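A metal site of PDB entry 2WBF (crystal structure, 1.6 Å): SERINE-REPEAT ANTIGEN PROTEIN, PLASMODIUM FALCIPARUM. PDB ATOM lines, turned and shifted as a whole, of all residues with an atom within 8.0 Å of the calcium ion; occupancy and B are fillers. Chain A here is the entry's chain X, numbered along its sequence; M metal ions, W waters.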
ATOM      1  N   LYS A 175      -7.159  19.527   1.646  1.00  0.00           N
ATOM      2  CA  LYS A 175      -6.088  19.733   2.618  1.00  0.00           C
ATOM      3  C   LYS A 175      -5.023  20.595   1.939  1.00  0.00           C
ATOM      4  O   LYS A 175      -4.483  20.208   0.890  1.00  0.00           O
ATOM      5  CB  LYS A 175      -5.503  18.392   3.072  1.00  0.00           C
ATOM      6  CG  LYS A 175      -4.631  18.462   4.328  1.00  0.00           C
ATOM      7  CD  LYS A 175      -4.538  17.083   5.015  1.00  0.00           C
ATOM      8  CE  LYS A 175      -3.860  17.166   6.378  1.00  0.00           C
ATOM      9  NZ  LYS A 175      -3.674  15.822   7.003  1.00  0.00           N
ATOM     10  N   ALA A 176      -4.736  21.744   2.518  1.00  0.00           N
ATOM     11  CA  ALA A 176      -3.827  22.711   1.897  1.00  0.00           C
ATOM     12  C   ALA A 176      -2.466  22.066   1.586  1.00  0.00           C
ATOM     13  O   ALA A 176      -1.881  22.362   0.563  1.00  0.00           O
ATOM     14  CB  ALA A 176      -3.651  23.927   2.798  1.00  0.00           C
ATOM     15  N   GLU A 177      -1.977  21.198   2.456  1.00  0.00           N
ATOM     16  CA  GLU A 177      -0.669  20.581   2.226  1.00  0.00           C
ATOM     17  C   GLU A 177      -0.610  19.924   0.843  1.00  0.00           C
ATOM     18  O   GLU A 177       0.444  19.877   0.187  1.00  0.00           O
ATOM     19  CB  GLU A 177      -0.350  19.548   3.308  1.00  0.00           C
ATOM     20  CG  GLU A 177      -1.071  18.229   3.115  1.00  0.00           C
ATOM     21  CD  GLU A 177      -0.584  17.119   4.050  1.00  0.00           C
ATOM     22  OE1 GLU A 177       0.107  17.409   5.034  1.00  0.00           O
ATOM     23  OE2 GLU A 177      -0.894  15.952   3.785  1.00  0.00           O
ATOM     24  N   ASN A 178      -1.748  19.391   0.386  1.00  0.00           N
ATOM     25  CA  ASN A 178      -1.763  18.653  -0.869  1.00  0.00           C
ATOM     26  C   ASN A 178      -1.448  19.472  -2.121  1.00  0.00           C
ATOM     27  O   ASN A 178      -1.103  18.883  -3.143  1.00  0.00           O
ATOM     28  CB  ASN A 178      -3.096  17.906  -1.039  1.00  0.00           C
ATOM     29  CG  ASN A 178      -3.252  16.805  -0.052  1.00  0.00           C
ATOM     30  OD1 ASN A 178      -2.266  16.323   0.507  1.00  0.00           O
ATOM     31  ND2 ASN A 178      -4.481  16.399   0.207  1.00  0.00           N
ATOM     32  N   VAL A 179      -1.536  20.804  -2.037  1.00  0.00           N
ATOM     33  CA  VAL A 179      -1.226  21.644  -3.189  1.00  0.00           C
ATOM     34  C   VAL A 179       0.079  22.411  -2.964  1.00  0.00           C
ATOM     35  O   VAL A 179       0.389  23.331  -3.712  1.00  0.00           O
ATOM     36  CB  VAL A 179      -2.395  22.623  -3.549  1.00  0.00           C
ATOM     37  CG1 VAL A 179      -3.662  21.851  -3.867  1.00  0.00           C
ATOM     38  CG2 VAL A 179      -2.639  23.646  -2.416  1.00  0.00           C
ATOM     39  N   LEU A 192      -3.278  13.096  -7.558  1.00  0.00           N
ATOM     40  CA  LEU A 192      -2.850  12.710  -6.228  1.00  0.00           C
ATOM     41  C   LEU A 192      -4.027  12.378  -5.358  1.00  0.00           C
ATOM     42  O   LEU A 192      -5.169  12.635  -5.732  1.00  0.00           O
ATOM     43  CB  LEU A 192      -2.050  13.839  -5.578  1.00  0.00           C
ATOM     44  CG  LEU A 192      -2.835  15.093  -5.153  1.00  0.00           C
ATOM     45  CD1 LEU A 192      -1.978  15.938  -4.204  1.00  0.00           C
ATOM     46  CD2 LEU A 192      -3.270  15.923  -6.342  1.00  0.00           C
ATOM     47  N   CYS A 193      -3.717  11.821  -4.195  1.00  0.00           N
ATOM     48  CA  CYS A 193      -4.705  11.461  -3.206  1.00  0.00           C
ATOM     49  C   CYS A 193      -5.003  12.623  -2.284  1.00  0.00           C
ATOM     50  O   CYS A 193      -4.180  13.522  -2.111  1.00  0.00           O
ATOM     51  CB  CYS A 193      -4.205  10.315  -2.320  1.00  0.00           C
ATOM     52  SG  CYS A 193      -3.610   8.863  -3.214  1.00  0.00           S
ATOM     53  N   GLY A 194      -6.180  12.580  -1.688  1.00  0.00           N
ATOM     54  CA  GLY A 194      -6.496  13.474  -0.591  1.00  0.00           C
ATOM     55  C   GLY A 194      -6.127  12.794   0.721  1.00  0.00           C
ATOM     56  O   GLY A 194      -5.481  11.733   0.736  1.00  0.00           O
ATOM     57  N   ASP A 195      -6.557  13.432   1.801  1.00  0.00           N
ATOM     58  CA  ASP A 195      -6.307  12.898   3.135  1.00  0.00           C
ATOM     59  C   ASP A 195      -7.643  12.624   3.819  1.00  0.00           C
ATOM     60  O   ASP A 195      -8.707  12.880   3.256  1.00  0.00           O
ATOM     61  CB  ASP A 195      -5.502  13.900   3.942  1.00  0.00           C
ATOM     62  CG  ASP A 195      -4.127  14.146   3.352  1.00  0.00           C
ATOM     63  OD1 ASP A 195      -3.251  13.288   3.529  1.00  0.00           O
ATOM     64  OD2 ASP A 195      -3.924  15.199   2.710  1.00  0.00           O
ATOM     65  N   ASP A 196      -7.558  12.090   5.038  1.00  0.00           N
ATOM     66  CA  ASP A 196      -8.737  11.764   5.816  1.00  0.00           C
ATOM     67  C   ASP A 196      -9.552  13.030   6.089  1.00  0.00           C
ATOM     68  O   ASP A 196     -10.756  12.967   6.218  1.00  0.00           O
ATOM     69  CB  ASP A 196      -8.264  11.154   7.153  1.00  0.00           C
ATOM     70  CG  ASP A 196      -9.319  10.353   7.849  1.00  0.00           C
ATOM     71  OD1 ASP A 196     -10.424  10.131   7.299  1.00  0.00           O
ATOM     72  OD2 ASP A 196      -9.030   9.912   8.980  1.00  0.00           O
ATOM     73  N   THR A 197      -8.891  14.185   6.196  1.00  0.00           N
ATOM     74  CA  THR A 197      -9.548  15.441   6.555  1.00  0.00           C
ATOM     75  C   THR A 197      -9.172  16.561   5.581  1.00  0.00           C
ATOM     76  O   THR A 197      -8.359  16.365   4.671  1.00  0.00           O
ATOM     77  CB  THR A 197      -9.153  15.893   7.955  1.00  0.00           C
ATOM     78  OG1 THR A 197      -7.745  16.128   7.979  1.00  0.00           O
ATOM     79  CG2 THR A 197      -9.492  14.811   8.993  1.00  0.00           C
ATOM     80  N   PHE A 251      -8.851  13.564  -3.621  1.00  0.00           N
ATOM     81  CA  PHE A 251      -8.285  14.904  -3.409  1.00  0.00           C
ATOM     82  C   PHE A 251      -9.367  15.904  -2.966  1.00  0.00           C
ATOM     83  O   PHE A 251      -9.118  16.768  -2.130  1.00  0.00           O
ATOM     84  CB  PHE A 251      -7.589  15.384  -4.691  1.00  0.00           C
ATOM     85  CG  PHE A 251      -7.117  16.815  -4.595  1.00  0.00           C
ATOM     86  CD1 PHE A 251      -5.923  17.132  -3.969  1.00  0.00           C
ATOM     87  CD2 PHE A 251      -7.888  17.838  -5.134  1.00  0.00           C
ATOM     88  CE1 PHE A 251      -5.504  18.451  -3.883  1.00  0.00           C
ATOM     89  CE2 PHE A 251      -7.475  19.163  -5.063  1.00  0.00           C
ATOM     90  CZ  PHE A 251      -6.284  19.472  -4.433  1.00  0.00           C
HETATM   91 CA    CA M   1      -1.634  14.574   1.975  1.00  0.00          CA
HETATM   92  O   HOH W   1      -0.307  12.647   2.999  1.00  0.00           O
HETATM   93  O   HOH W   2      -2.008  13.202  -0.153  1.00  0.00           O
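Within 4 Å of the calcium ion: Glu 177, Asn 178 and Asp 195. The nearest printed residue that does not touch the calcium ion is Lys 175 (4.9 Å).
The calcium ion is bound by the side-chain amide oxygen (OD1) of Asn 178 (2.4 Å), the side-chain carboxylate (OE2) of Glu 177 (2.4 Å), the side-chain carboxylate (OD2) of Asp 195 (2.5 Å), water W1 (2.6 Å), water W2 (2.6 Å) and the side-chain carboxylate (OD1) of Asp 195 (2.6 Å).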
